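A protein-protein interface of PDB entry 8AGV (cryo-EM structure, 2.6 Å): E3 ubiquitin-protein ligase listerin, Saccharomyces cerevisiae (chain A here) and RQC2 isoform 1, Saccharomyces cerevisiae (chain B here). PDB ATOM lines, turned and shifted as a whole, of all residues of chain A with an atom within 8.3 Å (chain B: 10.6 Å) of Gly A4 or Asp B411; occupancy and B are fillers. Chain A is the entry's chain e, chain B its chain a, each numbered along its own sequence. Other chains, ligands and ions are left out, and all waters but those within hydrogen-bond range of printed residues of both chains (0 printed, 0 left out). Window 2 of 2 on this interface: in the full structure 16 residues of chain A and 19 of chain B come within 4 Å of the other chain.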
ATOM      1  N   SER A   2      26.872  -5.677 -27.657  1.00  0.00           N
ATOM      2  CA  SER A   2      27.580  -6.411 -28.694  1.00  0.00           C
ATOM      3  C   SER A   2      28.040  -7.762 -28.171  1.00  0.00           C
ATOM      4  O   SER A   2      28.076  -8.738 -28.915  1.00  0.00           O
ATOM      5  CB  SER A   2      28.773  -5.601 -29.200  1.00  0.00           C
ATOM      6  OG  SER A   2      29.489  -6.312 -30.194  1.00  0.00           O
ATOM      7  N   PHE A   3      28.386  -7.823 -26.893  1.00  0.00           N
ATOM      8  CA  PHE A   3      28.815  -9.078 -26.291  1.00  0.00           C
ATOM      9  C   PHE A   3      27.830  -9.435 -25.196  1.00  0.00           C
ATOM     10  O   PHE A   3      27.450  -8.576 -24.406  1.00  0.00           O
ATOM     11  CB  PHE A   3      30.222  -8.949 -25.716  1.00  0.00           C
ATOM     12  CG  PHE A   3      31.275  -8.638 -26.738  1.00  0.00           C
ATOM     13  CD1 PHE A   3      31.907  -9.656 -27.428  1.00  0.00           C
ATOM     14  CD2 PHE A   3      31.644  -7.331 -27.000  1.00  0.00           C
ATOM     15  CE1 PHE A   3      32.883  -9.376 -28.363  1.00  0.00           C
ATOM     16  CE2 PHE A   3      32.616  -7.042 -27.935  1.00  0.00           C
ATOM     17  CZ  PHE A   3      33.239  -8.066 -28.617  1.00  0.00           C
ATOM     18  N   GLY A   4      27.401 -10.690 -25.138  1.00  0.00           N
ATOM     19  CA  GLY A   4      26.390 -11.068 -24.165  1.00  0.00           C
ATOM     20  C   GLY A   4      26.742 -12.240 -23.278  1.00  0.00           C
ATOM     21  O   GLY A   4      27.548 -13.084 -23.655  1.00  0.00           O
ATOM     22  N   GLY A   5      26.140 -12.298 -22.093  1.00  0.00           N
ATOM     23  CA  GLY A   5      26.399 -13.389 -21.169  1.00  0.00           C
ATOM     24  C   GLY A   5      27.346 -13.084 -20.031  1.00  0.00           C
ATOM     25  O   GLY A   5      28.100 -12.120 -20.092  1.00  0.00           O
ATOM     26  N   ILE A   6      27.287 -13.885 -18.972  1.00  0.00           N
ATOM     27  CA  ILE A   6      28.155 -13.684 -17.815  1.00  0.00           C
ATOM     28  C   ILE A   6      28.830 -15.003 -17.458  1.00  0.00           C
ATOM     29  O   ILE A   6      28.199 -16.056 -17.532  1.00  0.00           O
ATOM     30  CB  ILE A   6      27.343 -13.193 -16.597  1.00  0.00           C
ATOM     31  CG1 ILE A   6      26.648 -11.863 -16.899  1.00  0.00           C
ATOM     32  CG2 ILE A   6      28.229 -13.017 -15.375  1.00  0.00           C
ATOM     33  CD1 ILE A   6      27.596 -10.689 -17.014  1.00  0.00           C
ATOM     34  N   ASN A   7      30.102 -14.964 -17.071  1.00  0.00           N
ATOM     35  CA  ASN A   7      30.785 -16.183 -16.642  1.00  0.00           C
ATOM     36  C   ASN A   7      30.482 -16.448 -15.181  1.00  0.00           C
ATOM     37  O   ASN A   7      31.344 -16.278 -14.323  1.00  0.00           O
ATOM     38  CB  ASN A   7      32.294 -16.053 -16.842  1.00  0.00           C
ATOM     39  CG  ASN A   7      32.720 -16.335 -18.267  1.00  0.00           C
ATOM     40  OD1 ASN A   7      32.201 -17.244 -18.913  1.00  0.00           O
ATOM     41  ND2 ASN A   7      33.685 -15.567 -18.759  1.00  0.00           N
ATOM     42  N   THR A   8      29.259 -16.877 -14.893  1.00  0.00           N
ATOM     43  CA  THR A   8      28.854 -17.128 -13.516  1.00  0.00           C
ATOM     44  C   THR A   8      29.655 -18.246 -12.871  1.00  0.00           C
ATOM     45  O   THR A   8      30.032 -18.148 -11.705  1.00  0.00           O
ATOM     46  CB  THR A   8      27.362 -17.481 -13.451  1.00  0.00           C
ATOM     47  OG1 THR A   8      26.701 -16.979 -14.619  1.00  0.00           O
ATOM     48  CG2 THR A   8      26.725 -16.875 -12.212  1.00  0.00           C
ATOM     49  N   PRO A  34      37.784 -14.548 -22.248  1.00  0.00           N
ATOM     50  CA  PRO A  34      37.454 -13.222 -21.728  1.00  0.00           C
ATOM     51  C   PRO A  34      35.978 -13.029 -21.439  1.00  0.00           C
ATOM     52  O   PRO A  34      35.136 -13.466 -22.221  1.00  0.00           O
ATOM     53  CB  PRO A  34      37.884 -12.292 -22.858  1.00  0.00           C
ATOM     54  CG  PRO A  34      38.969 -13.030 -23.546  1.00  0.00           C
ATOM     55  CD  PRO A  34      38.560 -14.473 -23.496  1.00  0.00           C
ATOM     56  N   ASP A  35      35.669 -12.374 -20.325  1.00  0.00           N
ATOM     57  CA  ASP A  35      34.282 -12.119 -19.961  1.00  0.00           C
ATOM     58  C   ASP A  35      33.648 -11.168 -20.962  1.00  0.00           C
ATOM     59  O   ASP A  35      34.289 -10.225 -21.416  1.00  0.00           O
ATOM     60  CB  ASP A  35      34.220 -11.513 -18.560  1.00  0.00           C
ATOM     61  CG  ASP A  35      32.851 -11.646 -17.924  1.00  0.00           C
ATOM     62  OD1 ASP A  35      32.345 -12.782 -17.825  1.00  0.00           O
ATOM     63  OD2 ASP A  35      32.282 -10.615 -17.513  1.00  0.00           O
ATOM     64  N   PRO A  36      32.375 -11.399 -21.298  1.00  0.00           N
ATOM     65  CA  PRO A  36      31.704 -10.553 -22.284  1.00  0.00           C
ATOM     66  C   PRO A  36      31.603  -9.090 -21.869  1.00  0.00           C
ATOM     67  O   PRO A  36      31.743  -8.214 -22.716  1.00  0.00           O
ATOM     68  CB  PRO A  36      30.319 -11.176 -22.371  1.00  0.00           C
ATOM     69  CG  PRO A  36      30.582 -12.625 -22.138  1.00  0.00           C
ATOM     70  CD  PRO A  36      31.630 -12.649 -21.064  1.00  0.00           C
ATOM     71  N   SER A  37      31.360  -8.827 -20.593  1.00  0.00           N
ATOM     72  CA  SER A  37      31.260  -7.455 -20.130  1.00  0.00           C
ATOM     73  C   SER A  37      32.569  -6.717 -20.348  1.00  0.00           C
ATOM     74  O   SER A  37      32.571  -5.557 -20.749  1.00  0.00           O
ATOM     75  CB  SER A  37      30.898  -7.416 -18.650  1.00  0.00           C
ATOM     76  OG  SER A  37      31.967  -7.891 -17.853  1.00  0.00           O
ATOM     77  N   LEU A  39      34.740  -7.359 -22.637  1.00  0.00           N
ATOM     78  CA  LEU A  39      34.855  -7.134 -24.070  1.00  0.00           C
ATOM     79  C   LEU A  39      34.034  -5.931 -24.496  1.00  0.00           C
ATOM     80  O   LEU A  39      34.458  -5.161 -25.350  1.00  0.00           O
ATOM     81  CB  LEU A  39      34.441  -8.383 -24.832  1.00  0.00           C
ATOM     82  CG  LEU A  39      35.370  -9.583 -24.663  1.00  0.00           C
ATOM     83  CD1 LEU A  39      34.708 -10.867 -25.135  1.00  0.00           C
ATOM     84  CD2 LEU A  39      36.680  -9.344 -25.393  1.00  0.00           C
ATOM     85  N   ASN A  40      32.855  -5.762 -23.915  1.00  0.00           N
ATOM     86  CA  ASN A  40      32.037  -4.591 -24.213  1.00  0.00           C
ATOM     87  C   ASN A  40      32.785  -3.351 -23.782  1.00  0.00           C
ATOM     88  O   ASN A  40      32.710  -2.317 -24.438  1.00  0.00           O
ATOM     89  CB  ASN A  40      30.708  -4.655 -23.469  1.00  0.00           C
ATOM     90  CG  ASN A  40      29.699  -5.549 -24.151  1.00  0.00           C
ATOM     91  OD1 ASN A  40      29.526  -5.495 -25.367  1.00  0.00           O
ATOM     92  ND2 ASN A  40      29.008  -6.362 -23.365  1.00  0.00           N
ATOM     93  N   LYS B 403      20.309 -22.482 -12.975  1.00  0.00           N
ATOM     94  CA  LYS B 403      19.757 -22.153 -14.278  1.00  0.00           C
ATOM     95  C   LYS B 403      20.433 -20.926 -14.838  1.00  0.00           C
ATOM     96  O   LYS B 403      20.768 -20.879 -16.017  1.00  0.00           O
ATOM     97  CB  LYS B 403      18.268 -21.870 -14.166  1.00  0.00           C
ATOM     98  CG  LYS B 403      17.418 -23.063 -13.784  1.00  0.00           C
ATOM     99  CD  LYS B 403      16.040 -22.574 -13.387  1.00  0.00           C
ATOM    100  CE  LYS B 403      15.614 -21.451 -14.315  1.00  0.00           C
ATOM    101  NZ  LYS B 403      14.490 -20.659 -13.752  1.00  0.00           N
ATOM    102  N   LEU B 404      20.652 -19.934 -13.987  1.00  0.00           N
ATOM    103  CA  LEU B 404      21.272 -18.704 -14.442  1.00  0.00           C
ATOM    104  C   LEU B 404      22.669 -18.978 -14.949  1.00  0.00           C
ATOM    105  O   LEU B 404      23.097 -18.410 -15.949  1.00  0.00           O
ATOM    106  CB  LEU B 404      21.319 -17.677 -13.317  1.00  0.00           C
ATOM    107  CG  LEU B 404      19.963 -17.136 -12.871  1.00  0.00           C
ATOM    108  CD1 LEU B 404      20.119 -16.193 -11.689  1.00  0.00           C
ATOM    109  CD2 LEU B 404      19.254 -16.451 -14.028  1.00  0.00           C
ATOM    110  N   ALA B 405      23.388 -19.848 -14.256  1.00  0.00           N
ATOM    111  CA  ALA B 405      24.748 -20.133 -14.655  1.00  0.00           C
ATOM    112  C   ALA B 405      24.804 -20.750 -16.040  1.00  0.00           C
ATOM    113  O   ALA B 405      25.597 -20.328 -16.882  1.00  0.00           O
ATOM    114  CB  ALA B 405      25.401 -21.046 -13.640  1.00  0.00           C
ATOM    115  N   VAL B 406      23.932 -21.715 -16.299  1.00  0.00           N
ATOM    116  CA  VAL B 406      23.915 -22.352 -17.605  1.00  0.00           C
ATOM    117  C   VAL B 406      23.532 -21.336 -18.655  1.00  0.00           C
ATOM    118  O   VAL B 406      24.127 -21.283 -19.730  1.00  0.00           O
ATOM    119  CB  VAL B 406      22.924 -23.519 -17.648  1.00  0.00           C
ATOM    120  CG1 VAL B 406      23.054 -24.278 -18.959  1.00  0.00           C
ATOM    121  CG2 VAL B 406      23.164 -24.454 -16.481  1.00  0.00           C
ATOM    122  N   GLN B 407      22.567 -20.490 -18.330  1.00  0.00           N
ATOM    123  CA  GLN B 407      22.085 -19.523 -19.300  1.00  0.00           C
ATOM    124  C   GLN B 407      23.187 -18.579 -19.718  1.00  0.00           C
ATOM    125  O   GLN B 407      23.282 -18.220 -20.882  1.00  0.00           O
ATOM    126  CB  GLN B 407      20.905 -18.737 -18.736  1.00  0.00           C
ATOM    127  CG  GLN B 407      20.113 -17.983 -19.787  1.00  0.00           C
ATOM    128  CD  GLN B 407      19.471 -18.910 -20.800  1.00  0.00           C
ATOM    129  OE1 GLN B 407      19.598 -18.711 -22.007  1.00  0.00           O
ATOM    130  NE2 GLN B 407      18.785 -19.937 -20.312  1.00  0.00           N
ATOM    131  N   GLY B 408      24.032 -18.179 -18.780  1.00  0.00           N
ATOM    132  CA  GLY B 408      25.066 -17.221 -19.104  1.00  0.00           C
ATOM    133  C   GLY B 408      25.991 -17.776 -20.156  1.00  0.00           C
ATOM    134  O   GLY B 408      26.379 -17.067 -21.084  1.00  0.00           O
ATOM    135  N   LEU B 409      26.342 -19.049 -20.035  1.00  0.00           N
ATOM    136  CA  LEU B 409      27.181 -19.673 -21.050  1.00  0.00           C
ATOM    137  C   LEU B 409      26.482 -19.715 -22.399  1.00  0.00           C
ATOM    138  O   LEU B 409      27.101 -19.468 -23.430  1.00  0.00           O
ATOM    139  CB  LEU B 409      27.593 -21.080 -20.630  1.00  0.00           C
ATOM    140  CG  LEU B 409      28.825 -21.239 -19.740  1.00  0.00           C
ATOM    141  CD1 LEU B 409      29.956 -20.382 -20.276  1.00  0.00           C
ATOM    142  CD2 LEU B 409      28.533 -20.881 -18.294  1.00  0.00           C
ATOM    143  N   ILE B 410      25.191 -20.025 -22.396  1.00  0.00           N
ATOM    144  CA  ILE B 410      24.427 -20.074 -23.637  1.00  0.00           C
ATOM    145  C   ILE B 410      24.383 -18.704 -24.287  1.00  0.00           C
ATOM    146  O   ILE B 410      24.505 -18.583 -25.502  1.00  0.00           O
ATOM    147  CB  ILE B 410      22.998 -20.571 -23.378  1.00  0.00           C
ATOM    148  CG1 ILE B 410      23.028 -21.966 -22.761  1.00  0.00           C
ATOM    149  CG2 ILE B 410      22.183 -20.599 -24.661  1.00  0.00           C
ATOM    150  CD1 ILE B 410      21.654 -22.520 -22.468  1.00  0.00           C
ATOM    151  N   ASP B 411      24.237 -17.662 -23.480  1.00  0.00           N
ATOM    152  CA  ASP B 411      24.166 -16.306 -24.005  1.00  0.00           C
ATOM    153  C   ASP B 411      25.445 -15.944 -24.720  1.00  0.00           C
ATOM    154  O   ASP B 411      25.416 -15.254 -25.732  1.00  0.00           O
ATOM    155  CB  ASP B 411      23.896 -15.313 -22.886  1.00  0.00           C
ATOM    156  CG  ASP B 411      22.530 -15.502 -22.262  1.00  0.00           C
ATOM    157  OD1 ASP B 411      21.699 -16.217 -22.860  1.00  0.00           O
ATOM    158  OD2 ASP B 411      22.286 -14.939 -21.176  1.00  0.00           O
ATOM    159  N   GLN B 412      26.571 -16.408 -24.201  1.00  0.00           N
ATOM    160  CA  GLN B 412      27.852 -16.144 -24.836  1.00  0.00           C
ATOM    161  C   GLN B 412      27.902 -16.786 -26.209  1.00  0.00           C
ATOM    162  O   GLN B 412      28.685 -16.375 -27.060  1.00  0.00           O
ATOM    163  CB  GLN B 412      28.990 -16.658 -23.971  1.00  0.00           C
ATOM    164  CG  GLN B 412      28.766 -16.400 -22.498  1.00  0.00           C
ATOM    165  CD  GLN B 412      30.025 -16.561 -21.683  1.00  0.00           C
ATOM    166  OE1 GLN B 412      31.078 -16.928 -22.203  1.00  0.00           O
ATOM    167  NE2 GLN B 412      29.926 -16.276 -20.398  1.00  0.00           N
ATOM    168  N   GLN B 413      27.076 -17.802 -26.428  1.00  0.00           N
ATOM    169  CA  GLN B 413      27.071 -18.499 -27.706  1.00  0.00           C
ATOM    170  C   GLN B 413      28.188 -19.510 -27.786  1.00  0.00           C
ATOM    171  O   GLN B 413      28.617 -19.886 -28.873  1.00  0.00           O
ATOM    172  CB  GLN B 413      27.150 -17.511 -28.863  1.00  0.00           C
ATOM    173  CG  GLN B 413      25.829 -16.828 -29.179  1.00  0.00           C
ATOM    174  CD  GLN B 413      25.811 -16.213 -30.562  1.00  0.00           C
ATOM    175  OE1 GLN B 413      24.848 -15.552 -30.947  1.00  0.00           O
ATOM    176  NE2 GLN B 413      26.878 -16.431 -31.322  1.00  0.00           N
ATOM    177  N   MET B 414      28.677 -19.941 -26.634  1.00  0.00           N
ATOM    178  CA  MET B 414      29.721 -20.948 -26.601  1.00  0.00           C
ATOM    179  C   MET B 414      29.219 -22.273 -27.146  1.00  0.00           C
ATOM    180  O   MET B 414      28.040 -22.596 -27.019  1.00  0.00           O
ATOM    181  CB  MET B 414      30.229 -21.123 -25.174  1.00  0.00           C
ATOM    182  CG  MET B 414      31.422 -22.050 -25.050  1.00  0.00           C
ATOM    183  SD  MET B 414      32.076 -22.085 -23.372  1.00  0.00           S
ATOM    184  CE  MET B 414      32.370 -20.340 -23.102  1.00  0.00           C
ATOM    185  N   ASP B 415      30.110 -23.045 -27.751  1.00  0.00           N
ATOM    186  CA  ASP B 415      29.727 -24.325 -28.327  1.00  0.00           C
ATOM    187  C   ASP B 415      29.204 -25.184 -27.210  1.00  0.00           C
ATOM    188  O   ASP B 415      29.751 -25.187 -26.116  1.00  0.00           O
ATOM    189  CB  ASP B 415      30.958 -24.980 -28.956  1.00  0.00           C
ATOM    190  CG  ASP B 415      30.623 -26.162 -29.860  1.00  0.00           C
ATOM    191  OD1 ASP B 415      29.583 -26.824 -29.670  1.00  0.00           O
ATOM    192  OD2 ASP B 415      31.430 -26.441 -30.770  1.00  0.00           O
ATOM    193  N   TRP B 416      28.159 -25.946 -27.484  1.00  0.00           N
ATOM    194  CA  TRP B 416      27.550 -26.759 -26.449  1.00  0.00           C
ATOM    195  C   TRP B 416      28.534 -27.778 -25.906  1.00  0.00           C
ATOM    196  O   TRP B 416      28.574 -28.029 -24.705  1.00  0.00           O
ATOM    197  CB  TRP B 416      26.308 -27.445 -26.999  1.00  0.00           C
ATOM    198  CG  TRP B 416      25.201 -26.490 -27.317  1.00  0.00           C
ATOM    199  CD1 TRP B 416      25.152 -25.159 -27.016  1.00  0.00           C
ATOM    200  CD2 TRP B 416      23.975 -26.793 -27.987  1.00  0.00           C
ATOM    201  NE1 TRP B 416      23.975 -24.616 -27.463  1.00  0.00           N
ATOM    202  CE2 TRP B 416      23.234 -25.599 -28.061  1.00  0.00           C
ATOM    203  CE3 TRP B 416      23.431 -27.959 -28.531  1.00  0.00           C
ATOM    204  CZ2 TRP B 416      21.981 -25.538 -28.659  1.00  0.00           C
ATOM    205  CZ3 TRP B 416      22.191 -27.895 -29.123  1.00  0.00           C
ATOM    206  CH2 TRP B 416      21.479 -26.693 -29.184  1.00  0.00           C
ATOM    207  N   ILE B 419      30.888 -26.155 -23.534  1.00  0.00           N
ATOM    208  CA  ILE B 419      30.246 -25.843 -22.273  1.00  0.00           C
ATOM    209  C   ILE B 419      30.291 -27.070 -21.382  1.00  0.00           C
ATOM    210  O   ILE B 419      30.631 -26.975 -20.207  1.00  0.00           O
ATOM    211  CB  ILE B 419      28.782 -25.410 -22.481  1.00  0.00           C
ATOM    212  CG1 ILE B 419      28.716 -24.086 -23.238  1.00  0.00           C
ATOM    213  CG2 ILE B 419      28.054 -25.270 -21.153  1.00  0.00           C
ATOM    214  CD1 ILE B 419      27.308 -23.652 -23.581  1.00  0.00           C
ATOM    215  N   LEU B 443      20.758 -29.580 -24.200  1.00  0.00           N
ATOM    216  CA  LEU B 443      20.678 -28.176 -24.579  1.00  0.00           C
ATOM    217  C   LEU B 443      19.773 -27.977 -25.775  1.00  0.00           C
ATOM    218  O   LEU B 443      19.156 -26.927 -25.921  1.00  0.00           O
ATOM    219  CB  LEU B 443      22.068 -27.591 -24.813  1.00  0.00           C
ATOM    220  CG  LEU B 443      22.879 -27.468 -23.522  1.00  0.00           C
ATOM    221  CD1 LEU B 443      24.211 -26.781 -23.767  1.00  0.00           C
ATOM    222  CD2 LEU B 443      22.076 -26.714 -22.475  1.00  0.00           C
ATOM    223  N   ASN B 446      16.792 -27.555 -24.473  1.00  0.00           N
ATOM    224  CA  ASN B 446      16.903 -26.593 -23.372  1.00  0.00           C
ATOM    225  C   ASN B 446      16.546 -27.195 -22.034  1.00  0.00           C
ATOM    226  O   ASN B 446      15.934 -26.538 -21.197  1.00  0.00           O
ATOM    227  CB  ASN B 446      16.089 -25.324 -23.628  1.00  0.00           C
ATOM    228  CG  ASN B 446      16.943 -24.184 -24.137  1.00  0.00           C
ATOM    229  OD1 ASN B 446      18.126 -24.360 -24.420  1.00  0.00           O
ATOM    230  ND2 ASN B 446      16.346 -23.005 -24.250  1.00  0.00           N
ATOM    231  N   LEU B 510      15.219 -24.637 -19.000  1.00  0.00           N
ATOM    232  CA  LEU B 510      15.935 -23.411 -18.726  1.00  0.00           C
ATOM    233  C   LEU B 510      15.012 -22.210 -18.780  1.00  0.00           C
ATOM    234  O   LEU B 510      15.107 -21.315 -17.945  1.00  0.00           O
ATOM    235  CB  LEU B 510      17.090 -23.253 -19.703  1.00  0.00           C
ATOM    236  CG  LEU B 510      18.273 -24.140 -19.337  1.00  0.00           C
ATOM    237  CD1 LEU B 510      19.114 -24.476 -20.554  1.00  0.00           C
ATOM    238  CD2 LEU B 510      19.100 -23.462 -18.258  1.00  0.00           C
ATOM    239  N   GLY B 511      14.114 -22.184 -19.756  1.00  0.00           N
ATOM    240  CA  GLY B 511      13.220 -21.052 -19.898  1.00  0.00           C
ATOM    241  C   GLY B 511      12.258 -20.833 -18.750  1.00  0.00           C
ATOM    242  O   GLY B 511      12.063 -19.702 -18.309  1.00  0.00           O
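Gly A4 touches Asp B411. Gln B412 touches Gly A4. Gly B408 touches Gly A5. Gly A5 touches Asp B411. Ile A6 touches Gly B408 (O to CA, 3.7 Å). Thr A8 touches Ala B405.
Printed residues of chain B that touch a printed residue of chain A: Ala B405, Gly B408, Asp B411 and Gln B412. Of the 13 printed residues of chain A, 5 touch a printed residue of chain B. Printed residues of chain A that touch a printed residue of chain B: Gly A4, Gly A5, Ile A6, Asn A7 and Thr A8.
The side-chain amide nitrogen (NE2) of Gln B412 is in hydrogen-bond range of the backbone carbonyl oxygen (O) of Ile A6, at 3.4 Å. The side-chain amide nitrogen (NE2) of Gln B412 sits at hydrogen-bond distance from the side-chain amide oxygen (OD1) of Asn A7, at 2.9 Å.
OE1 of Gln B407 lies close to OD1 of Asp B411. The side-chain hydroxyl (OG1) of Thr A8 lies within hydrogen-bond range of the backbone carbonyl oxygen (O) of Ile A6, 3.4 Å away. OD1 of Asp A35 sits at hydrogen-bond distance from N of Asn A7, at 3.2 Å.
Gly A4 touches two residues of chain B. Gly A5 touches two residues of chain B. Printed residues of chain B within 4 Å of Asn A7: Gln B412. Of the printed residues of chain B, Thr A8 touches Ala B405 (3.7 Å). Leu B404 touches none of the printed residues of chain A. Of the printed residues of chain A, Gly B408 touches Gly A5 (3.7 Å) and Ile A6 (3.7 Å). Asp B411 touches two residues of chain A. Asp B415 touches none of the printed residues of chain A. The nearest residue of chain A that does not touch Asp B411 is Ile A6 (5.4 Å).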
